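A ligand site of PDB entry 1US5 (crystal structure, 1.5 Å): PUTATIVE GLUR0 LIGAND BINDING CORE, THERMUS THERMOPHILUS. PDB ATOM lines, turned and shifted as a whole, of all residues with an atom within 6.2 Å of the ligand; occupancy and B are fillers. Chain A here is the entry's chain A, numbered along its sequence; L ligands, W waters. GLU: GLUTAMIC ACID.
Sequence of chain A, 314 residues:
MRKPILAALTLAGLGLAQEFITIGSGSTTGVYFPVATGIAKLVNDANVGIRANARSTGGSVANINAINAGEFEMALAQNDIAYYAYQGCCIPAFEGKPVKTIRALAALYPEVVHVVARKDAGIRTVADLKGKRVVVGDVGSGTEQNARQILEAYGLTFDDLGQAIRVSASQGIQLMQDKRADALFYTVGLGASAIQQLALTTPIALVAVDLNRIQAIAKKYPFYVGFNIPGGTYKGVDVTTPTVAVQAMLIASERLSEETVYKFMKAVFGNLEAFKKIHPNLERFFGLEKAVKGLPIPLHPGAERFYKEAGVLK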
ATOM      1  N   SER A  25      -4.981  28.127 -26.027  1.00  0.00           N
ATOM      2  CA  SER A  25      -5.809  29.181 -25.452  1.00  0.00           C
ATOM      3  C   SER A  25      -6.924  28.667 -24.540  1.00  0.00           C
ATOM      4  O   SER A  25      -6.653  28.231 -23.420  1.00  0.00           O
ATOM      5  CB  SER A  25      -6.388  30.070 -26.573  1.00  0.00           C
ATOM      6  OG  SER A  25      -7.184  29.332 -27.499  1.00  0.00           O
ATOM      7  N   GLY A  26      -8.168  28.738 -25.004  1.00  0.00           N
ATOM      8  CA  GLY A  26      -9.282  28.274 -24.184  1.00  0.00           C
ATOM      9  C   GLY A  26     -10.520  28.102 -25.031  1.00  0.00           C
ATOM     10  O   GLY A  26     -10.416  27.868 -26.235  1.00  0.00           O
ATOM     11  N   SER A  27     -11.695  28.216 -24.417  1.00  0.00           N
ATOM     12  CA  SER A  27     -12.949  28.081 -25.146  1.00  0.00           C
ATOM     13  C   SER A  27     -13.048  29.194 -26.181  1.00  0.00           C
ATOM     14  O   SER A  27     -12.562  30.300 -25.954  1.00  0.00           O
ATOM     15  CB  SER A  27     -14.145  28.161 -24.201  1.00  0.00           C
ATOM     16  OG  SER A  27     -14.227  26.997 -23.383  1.00  0.00           O
ATOM     17  N   GLY A  30     -14.317  32.484 -24.769  1.00  0.00           N
ATOM     18  CA  GLY A  30     -13.660  33.062 -23.616  1.00  0.00           C
ATOM     19  C   GLY A  30     -12.823  34.230 -24.115  1.00  0.00           C
ATOM     20  O   GLY A  30     -13.110  34.766 -25.195  1.00  0.00           O
ATOM     21  N   VAL A  31     -11.807  34.638 -23.367  1.00  0.00           N
ATOM     22  CA  VAL A  31     -10.954  35.746 -23.788  1.00  0.00           C
ATOM     23  C   VAL A  31      -9.608  35.268 -24.354  1.00  0.00           C
ATOM     24  O   VAL A  31      -9.047  35.897 -25.249  1.00  0.00           O
ATOM     25  CB  VAL A  31     -10.720  36.734 -22.624  1.00  0.00           C
ATOM     26  CG1 VAL A  31      -9.763  37.856 -23.045  1.00  0.00           C
ATOM     27  CG2 VAL A  31     -12.051  37.328 -22.188  1.00  0.00           C
ATOM     28  N   TYR A  32      -9.080  34.156 -23.843  1.00  0.00           N
ATOM     29  CA  TYR A  32      -7.807  33.629 -24.341  1.00  0.00           C
ATOM     30  C   TYR A  32      -7.846  33.394 -25.850  1.00  0.00           C
ATOM     31  O   TYR A  32      -6.903  33.754 -26.562  1.00  0.00           O
ATOM     32  CB  TYR A  32      -7.480  32.279 -23.705  1.00  0.00           C
ATOM     33  CG  TYR A  32      -6.931  32.266 -22.302  1.00  0.00           C
ATOM     34  CD1 TYR A  32      -6.780  33.443 -21.553  1.00  0.00           C
ATOM     35  CD2 TYR A  32      -6.583  31.064 -21.698  1.00  0.00           C
ATOM     36  CE1 TYR A  32      -6.288  33.402 -20.243  1.00  0.00           C
ATOM     37  CE2 TYR A  32      -6.088  31.009 -20.402  1.00  0.00           C
ATOM     38  CZ  TYR A  32      -5.951  32.172 -19.684  1.00  0.00           C
ATOM     39  OH  TYR A  32      -5.485  32.082 -18.385  1.00  0.00           O
ATOM     40  N   PHE A  33      -8.917  32.767 -26.329  1.00  0.00           N
ATOM     41  CA  PHE A  33      -9.016  32.452 -27.752  1.00  0.00           C
ATOM     42  C   PHE A  33      -8.941  33.661 -28.673  1.00  0.00           C
ATOM     43  O   PHE A  33      -8.136  33.675 -29.598  1.00  0.00           O
ATOM     44  CB  PHE A  33     -10.281  31.643 -28.033  1.00  0.00           C
ATOM     45  CG  PHE A  33     -10.365  31.138 -29.433  1.00  0.00           C
ATOM     46  CD1 PHE A  33      -9.565  30.076 -29.861  1.00  0.00           C
ATOM     47  CD2 PHE A  33     -11.201  31.755 -30.360  1.00  0.00           C
ATOM     48  CE1 PHE A  33      -9.601  29.642 -31.183  1.00  0.00           C
ATOM     49  CE2 PHE A  33     -11.233  31.334 -31.681  1.00  0.00           C
ATOM     50  CZ  PHE A  33     -10.433  30.279 -32.101  1.00  0.00           C
ATOM     51  N   GLY A  58      -8.989  23.345 -23.302  1.00  0.00           N
ATOM     52  CA  GLY A  58      -9.712  23.396 -22.046  1.00  0.00           C
ATOM     53  C   GLY A  58      -9.213  24.490 -21.108  1.00  0.00           C
ATOM     54  O   GLY A  58      -9.856  24.786 -20.101  1.00  0.00           O
ATOM     55  N   GLY A  59      -8.073  25.094 -21.422  1.00  0.00           N
ATOM     56  CA  GLY A  59      -7.568  26.142 -20.550  1.00  0.00           C
ATOM     57  C   GLY A  59      -6.154  25.944 -20.048  1.00  0.00           C
ATOM     58  O   GLY A  59      -5.386  25.142 -20.585  1.00  0.00           O
ATOM     59  N   SER A  60      -5.829  26.659 -18.967  1.00  0.00           N
ATOM     60  CA  SER A  60      -4.498  26.661 -18.363  1.00  0.00           C
ATOM     61  C   SER A  60      -3.780  25.356 -18.130  1.00  0.00           C
ATOM     62  O   SER A  60      -2.633  25.206 -18.555  1.00  0.00           O
ATOM     63  CB  SER A  60      -4.525  27.436 -17.036  1.00  0.00           C
ATOM     64  OG  SER A  60      -4.849  28.792 -17.249  1.00  0.00           O
ATOM     65  N   VAL A  61      -4.420  24.411 -17.442  1.00  0.00           N
ATOM     66  CA  VAL A  61      -3.765  23.146 -17.158  1.00  0.00           C
ATOM     67  C   VAL A  61      -3.457  22.386 -18.445  1.00  0.00           C
ATOM     68  O   VAL A  61      -2.351  21.897 -18.649  1.00  0.00           O
ATOM     69  CB  VAL A  61      -4.602  22.276 -16.203  1.00  0.00           C
ATOM     70  CG1 VAL A  61      -3.933  20.923 -15.986  1.00  0.00           C
ATOM     71  CG2 VAL A  61      -4.770  22.994 -14.869  1.00  0.00           C
ATOM     72  N   ASN A  63      -3.110  23.571 -21.399  1.00  0.00           N
ATOM     73  CA  ASN A  63      -2.087  24.303 -22.160  1.00  0.00           C
ATOM     74  C   ASN A  63      -0.680  24.026 -21.663  1.00  0.00           C
ATOM     75  O   ASN A  63       0.232  23.810 -22.455  1.00  0.00           O
ATOM     76  CB  ASN A  63      -2.348  25.808 -22.115  1.00  0.00           C
ATOM     77  CG  ASN A  63      -3.596  26.218 -22.850  1.00  0.00           C
ATOM     78  OD1 ASN A  63      -4.138  25.455 -23.658  1.00  0.00           O
ATOM     79  ND2 ASN A  63      -4.067  27.439 -22.592  1.00  0.00           N
ATOM     80  N   LEU A  76      -1.632  30.722 -23.379  1.00  0.00           N
ATOM     81  CA  LEU A  76      -2.089  31.703 -22.392  1.00  0.00           C
ATOM     82  C   LEU A  76      -2.375  30.842 -21.167  1.00  0.00           C
ATOM     83  O   LEU A  76      -2.852  29.714 -21.298  1.00  0.00           O
ATOM     84  CB  LEU A  76      -3.378  32.387 -22.853  1.00  0.00           C
ATOM     85  CG  LEU A  76      -3.297  33.505 -23.894  1.00  0.00           C
ATOM     86  CD1 LEU A  76      -2.457  34.644 -23.338  1.00  0.00           C
ATOM     87  CD2 LEU A  76      -2.697  32.987 -25.184  1.00  0.00           C
ATOM     88  N   ALA A  77      -2.086  31.353 -19.986  1.00  0.00           N
ATOM     89  CA  ALA A  77      -2.336  30.608 -18.758  1.00  0.00           C
ATOM     90  C   ALA A  77      -2.406  31.535 -17.562  1.00  0.00           C
ATOM     91  O   ALA A  77      -1.864  32.630 -17.588  1.00  0.00           O
ATOM     92  CB  ALA A  77      -1.228  29.564 -18.532  1.00  0.00           C
ATOM     93  N   GLN A  78      -3.079  31.086 -16.509  1.00  0.00           N
ATOM     94  CA  GLN A  78      -3.201  31.878 -15.284  1.00  0.00           C
ATOM     95  C   GLN A  78      -1.867  31.855 -14.555  1.00  0.00           C
ATOM     96  O   GLN A  78      -1.147  30.855 -14.586  1.00  0.00           O
ATOM     97  CB  GLN A  78      -4.288  31.288 -14.391  1.00  0.00           C
ATOM     98  CG  GLN A  78      -5.665  31.287 -15.044  1.00  0.00           C
ATOM     99  CD  GLN A  78      -6.734  30.623 -14.216  1.00  0.00           C
ATOM    100  OE1 GLN A  78      -7.833  30.379 -14.699  1.00  0.00           O
ATOM    101  NE2 GLN A  78      -6.435  30.340 -12.947  1.00  0.00           N
ATOM    102  N   ILE A  81      -1.699  28.973 -11.887  1.00  0.00           N
ATOM    103  CA  ILE A  81      -1.477  27.656 -12.468  1.00  0.00           C
ATOM    104  C   ILE A  81      -0.039  27.510 -12.985  1.00  0.00           C
ATOM    105  O   ILE A  81       0.571  26.451 -12.829  1.00  0.00           O
ATOM    106  CB  ILE A  81      -2.450  27.376 -13.639  1.00  0.00           C
ATOM    107  CG1 ILE A  81      -3.902  27.587 -13.176  1.00  0.00           C
ATOM    108  CG2 ILE A  81      -2.251  25.962 -14.169  1.00  0.00           C
ATOM    109  CD1 ILE A  81      -4.314  26.696 -12.011  1.00  0.00           C
ATOM    110  N   TYR A 109      -3.593  40.708 -18.296  1.00  0.00           N
ATOM    111  CA  TYR A 109      -4.743  41.375 -17.692  1.00  0.00           C
ATOM    112  C   TYR A 109      -5.315  40.517 -16.568  1.00  0.00           C
ATOM    113  O   TYR A 109      -4.965  39.343 -16.434  1.00  0.00           O
ATOM    114  CB  TYR A 109      -5.823  41.606 -18.765  1.00  0.00           C
ATOM    115  CG  TYR A 109      -6.319  40.338 -19.414  1.00  0.00           C
ATOM    116  CD1 TYR A 109      -7.302  39.550 -18.805  1.00  0.00           C
ATOM    117  CD2 TYR A 109      -5.753  39.874 -20.605  1.00  0.00           C
ATOM    118  CE1 TYR A 109      -7.709  38.328 -19.360  1.00  0.00           C
ATOM    119  CE2 TYR A 109      -6.149  38.664 -21.170  1.00  0.00           C
ATOM    120  CZ  TYR A 109      -7.119  37.890 -20.531  1.00  0.00           C
ATOM    121  OH  TYR A 109      -7.461  36.673 -21.067  1.00  0.00           O
ATOM    122  N   GLU A 111      -7.842  38.145 -14.517  1.00  0.00           N
ATOM    123  CA  GLU A 111      -8.849  37.146 -14.812  1.00  0.00           C
ATOM    124  C   GLU A 111      -9.676  37.029 -13.544  1.00  0.00           C
ATOM    125  O   GLU A 111      -9.187  36.599 -12.498  1.00  0.00           O
ATOM    126  CB  GLU A 111      -8.204  35.821 -15.168  1.00  0.00           C
ATOM    127  CG  GLU A 111      -7.482  35.871 -16.497  1.00  0.00           C
ATOM    128  CD  GLU A 111      -7.191  34.501 -17.044  1.00  0.00           C
ATOM    129  OE1 GLU A 111      -6.053  34.012 -16.859  1.00  0.00           O
ATOM    130  OE2 GLU A 111      -8.110  33.918 -17.645  1.00  0.00           O
ATOM    131  N   ASP A 138     -13.929  23.782 -17.537  1.00  0.00           N
ATOM    132  CA  ASP A 138     -13.683  22.767 -18.549  1.00  0.00           C
ATOM    133  C   ASP A 138     -12.625  21.785 -18.063  1.00  0.00           C
ATOM    134  O   ASP A 138     -11.908  22.038 -17.088  1.00  0.00           O
ATOM    135  CB  ASP A 138     -13.211  23.426 -19.842  1.00  0.00           C
ATOM    136  CG  ASP A 138     -13.475  22.579 -21.082  1.00  0.00           C
ATOM    137  OD1 ASP A 138     -13.905  21.415 -20.941  1.00  0.00           O
ATOM    138  OD2 ASP A 138     -13.255  23.088 -22.204  1.00  0.00           O
ATOM    139  N   GLY A 140      -9.261  20.324 -17.777  1.00  0.00           N
ATOM    140  CA  GLY A 140      -7.950  20.920 -17.988  1.00  0.00           C
ATOM    141  C   GLY A 140      -7.955  22.434 -17.844  1.00  0.00           C
ATOM    142  O   GLY A 140      -7.022  23.112 -18.278  1.00  0.00           O
ATOM    143  N   SER A 141      -9.009  22.976 -17.243  1.00  0.00           N
ATOM    144  CA  SER A 141      -9.107  24.419 -17.056  1.00  0.00           C
ATOM    145  C   SER A 141      -8.479  24.915 -15.768  1.00  0.00           C
ATOM    146  O   SER A 141      -8.316  24.167 -14.805  1.00  0.00           O
ATOM    147  CB  SER A 141     -10.584  24.840 -17.051  1.00  0.00           C
ATOM    148  OG  SER A 141     -11.244  24.343 -15.889  1.00  0.00           O
ATOM    149  N   GLY A 142      -8.117  26.200 -15.768  1.00  0.00           N
ATOM    150  CA  GLY A 142      -7.589  26.788 -14.558  1.00  0.00           C
ATOM    151  C   GLY A 142      -8.827  27.030 -13.696  1.00  0.00           C
ATOM    152  O   GLY A 142      -8.772  26.924 -12.469  1.00  0.00           O
ATOM    153  N   THR A 143      -9.948  27.316 -14.360  1.00  0.00           N
ATOM    154  CA  THR A 143     -11.227  27.574 -13.692  1.00  0.00           C
ATOM    155  C   THR A 143     -11.607  26.515 -12.666  1.00  0.00           C
ATOM    156  O   THR A 143     -11.997  26.834 -11.545  1.00  0.00           O
ATOM    157  CB  THR A 143     -12.384  27.654 -14.723  1.00  0.00           C
ATOM    158  OG1 THR A 143     -12.156  28.751 -15.609  1.00  0.00           O
ATOM    159  CG2 THR A 143     -13.732  27.828 -14.022  1.00  0.00           C
ATOM    160  N   GLU A 144     -11.487  25.248 -13.056  1.00  0.00           N
ATOM    161  CA  GLU A 144     -11.824  24.160 -12.167  1.00  0.00           C
ATOM    162  C   GLU A 144     -10.998  24.178 -10.896  1.00  0.00           C
ATOM    163  O   GLU A 144     -11.490  23.834  -9.823  1.00  0.00           O
ATOM    164  CB  GLU A 144     -11.641  22.821 -12.889  1.00  0.00           C
ATOM    165  CG  GLU A 144     -11.658  21.612 -11.960  1.00  0.00           C
ATOM    166  CD  GLU A 144     -11.494  20.297 -12.695  1.00  0.00           C
ATOM    167  OE1 GLU A 144     -10.718  20.260 -13.672  1.00  0.00           O
ATOM    168  OE2 GLU A 144     -12.139  19.312 -12.282  1.00  0.00           O
ATOM    169  N   ASN A 146      -9.621  26.917  -9.490  1.00  0.00           N
ATOM    170  CA  ASN A 146     -10.077  28.040  -8.675  1.00  0.00           C
ATOM    171  C   ASN A 146     -11.404  27.680  -8.005  1.00  0.00           C
ATOM    172  O   ASN A 146     -11.651  28.042  -6.865  1.00  0.00           O
ATOM    173  CB  ASN A 146     -10.259  29.296  -9.524  1.00  0.00           C
ATOM    174  CG  ASN A 146      -8.969  29.739 -10.197  1.00  0.00           C
ATOM    175  OD1 ASN A 146      -8.968  30.017 -11.390  1.00  0.00           O
ATOM    176  ND2 ASN A 146      -7.887  29.803  -9.436  1.00  0.00           N
ATOM    177  N   TYR A 186     -16.286  30.513 -13.913  1.00  0.00           N
ATOM    178  CA  TYR A 186     -15.435  30.841 -15.062  1.00  0.00           C
ATOM    179  C   TYR A 186     -14.406  31.866 -14.619  1.00  0.00           C
ATOM    180  O   TYR A 186     -14.763  32.978 -14.235  1.00  0.00           O
ATOM    181  CB  TYR A 186     -16.264  31.396 -16.239  1.00  0.00           C
ATOM    182  CG  TYR A 186     -15.601  31.252 -17.611  1.00  0.00           C
ATOM    183  CD1 TYR A 186     -14.409  30.551 -17.760  1.00  0.00           C
ATOM    184  CD2 TYR A 186     -16.210  31.761 -18.752  1.00  0.00           C
ATOM    185  CE1 TYR A 186     -13.840  30.354 -19.033  1.00  0.00           C
ATOM    186  CE2 TYR A 186     -15.658  31.578 -20.028  1.00  0.00           C
ATOM    187  CZ  TYR A 186     -14.471  30.868 -20.155  1.00  0.00           C
ATOM    188  OH  TYR A 186     -13.932  30.649 -21.412  1.00  0.00           O
ATOM    189  N   THR A 187     -13.131  31.481 -14.633  1.00  0.00           N
ATOM    190  CA  THR A 187     -12.065  32.406 -14.284  1.00  0.00           C
ATOM    191  C   THR A 187     -11.709  32.977 -15.634  1.00  0.00           C
ATOM    192  O   THR A 187     -11.101  32.303 -16.480  1.00  0.00           O
ATOM    193  CB  THR A 187     -10.861  31.673 -13.672  1.00  0.00           C
ATOM    194  OG1 THR A 187     -11.289  31.025 -12.468  1.00  0.00           O
ATOM    195  CG2 THR A 187      -9.737  32.664 -13.352  1.00  0.00           C
ATOM    196  N   VAL A 188     -12.092  34.229 -15.865  1.00  0.00           N
ATOM    197  CA  VAL A 188     -11.897  34.823 -17.177  1.00  0.00           C
ATOM    198  C   VAL A 188     -11.885  36.342 -17.121  1.00  0.00           C
ATOM    199  O   VAL A 188     -12.382  36.948 -16.177  1.00  0.00           O
ATOM    200  CB  VAL A 188     -13.042  34.333 -18.103  1.00  0.00           C
ATOM    201  CG1 VAL A 188     -14.382  34.870 -17.611  1.00  0.00           C
ATOM    202  CG2 VAL A 188     -12.792  34.751 -19.557  1.00  0.00           C
ATOM    203  N   GLY A 189     -11.292  36.960 -18.142  1.00  0.00           N
ATOM    204  CA  GLY A 189     -11.265  38.410 -18.186  1.00  0.00           C
ATOM    205  C   GLY A 189     -12.683  38.951 -18.279  1.00  0.00           C
ATOM    206  O   GLY A 189     -13.597  38.259 -18.755  1.00  0.00           O
HETATM  207  N   GLU L   1      -8.222  31.200 -17.279  1.00  0.00           N
HETATM  208  CA  GLU L   1      -9.205  30.209 -17.820  1.00  0.00           C
HETATM  209  C   GLU L   1      -8.710  28.779 -17.637  1.00  0.00           C
HETATM  210  O   GLU L   1      -7.476  28.574 -17.637  1.00  0.00           O
HETATM  211  CB  GLU L   1      -9.440  30.482 -19.313  1.00  0.00           C
HETATM  212  CG  GLU L   1     -10.033  31.850 -19.563  1.00  0.00           C
HETATM  213  CD  GLU L   1     -10.226  32.172 -21.028  1.00  0.00           C
HETATM  214  OE1 GLU L   1     -10.410  31.235 -21.837  1.00  0.00           O
HETATM  215  OE2 GLU L   1     -10.216  33.372 -21.378  1.00  0.00           O
HETATM  216  OXT GLU L   1      -9.558  27.886 -17.487  1.00  0.00           O
HETATM  217  O   HOH W   1      -9.350  35.281 -19.610  1.00  0.00           O
HETATM  218  O   HOH W   2     -10.758  31.553 -24.503  1.00  0.00           O
HETATM  219  O   HOH W   3     -11.780  28.997 -21.649  1.00  0.00           O
HETATM  220  O   HOH W   4     -11.299  27.194 -19.666  1.00  0.00           O
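Merely in contact with the ligand: Gly 26 (3.9 Å), Gly 30 (3.9 Å), Gly 59 (3.8 Å), Ser 141 (3.2 Å), Tyr 186 (3.6 Å) and Val 188 (3.4 Å). Hydrophobic or aromatic side chains within 4 Å of the ligand: Val 31, Tyr 32 and Val 188. Within 4 Å of the ligand: Gly 26, Gly 30, Val 31, Tyr 32, Gly 59, Ser 60, Gln 78, Glu 111, Ser 141, Gly 142, Thr 143, Tyr 186, Thr 187 and Val 188. The nearest printed residue that does not touch the ligand is Gly 58 (4.1 Å).
The side-chain hydroxyl of Tyr 32 is in hydrogen-bond range of the backbone NH of Gln 78 (3.2 Å). The side-chain amide nitrogen of Gln 78 sits at hydrogen-bond distance from the side-chain amide oxygen of Asn 146, at 3.0 Å. The side-chain carboxylate of Glu 111 sits at hydrogen-bond distance from the side-chain hydroxyl of Tyr 32, 2.5 Å away. The side-chain amide oxygen of Asn 146 lies close to the backbone carbonyl oxygen of Gly 142, 3.3 Å away. The side-chain amide oxygen of Asn 146 sits at hydrogen-bond distance from the side-chain hydroxyl of Thr 187 (2.8 Å). The backbone carbonyl oxygen of Gly 58 lies close to the backbone NH of Ser 141 (3.5 Å). OG of Ser 141 lies within hydrogen-bond range of N of Glu 144. The backbone carbonyl oxygen of Gly 59 sits close to the side-chain amide nitrogen of Asn 63 (3.3 Å).
Water W3 lies within hydrogen-bond range of OE1 of the ligand (2.6 Å), OH of Tyr 186 (2.7 Å) and N of Ser 27 (2.9 Å). Water W1 lies within hydrogen-bond range of OE2 of Glu 111 (2.7 Å), OE2 of the ligand (2.7 Å), OH of Tyr 109 (2.8 Å) and N of Gly 189 (3.0 Å). Water W4 bridges O of Gly 58 (2.8 Å) and OXT of the ligand (2.9 Å).
An oxygen (O) of the ligand sits at hydrogen-bond distance from the backbone NH (N) of Ser 60 (2.9 Å). An oxygen (O) of the ligand lies within hydrogen-bond range of the side-chain hydroxyl (OG) of Ser 60 (2.7 Å). The side-chain amide oxygen (OE1) of Gln 78 sits at hydrogen-bond distance from a nitrogen (N) of the ligand, 2.7 Å away. N of the ligand lies within salt-bridge range of OE2 of Glu 111 (2.7 Å). OXT of the ligand is in hydrogen-bond range of N of Gly 142 (2.8 Å). OE2 of the ligand is in hydrogen-bond range of N of Tyr 32 (2.8 Å). OH of Tyr 32 lies within hydrogen-bond range of N of the ligand (3.1 Å). The backbone NH (N) of Val 31 lies within hydrogen-bond range of an oxygen (OE2) of the ligand (2.8 Å). The backbone carbonyl oxygen of Thr 187 sits close to a nitrogen (N) of the ligand (3.2 Å). An oxygen (OXT) of the ligand sits at hydrogen-bond distance from the backbone NH of Thr 143, at 3.2 Å. OG1 of Thr 143 is in hydrogen-bond range of OXT of the ligand (3.3 Å).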
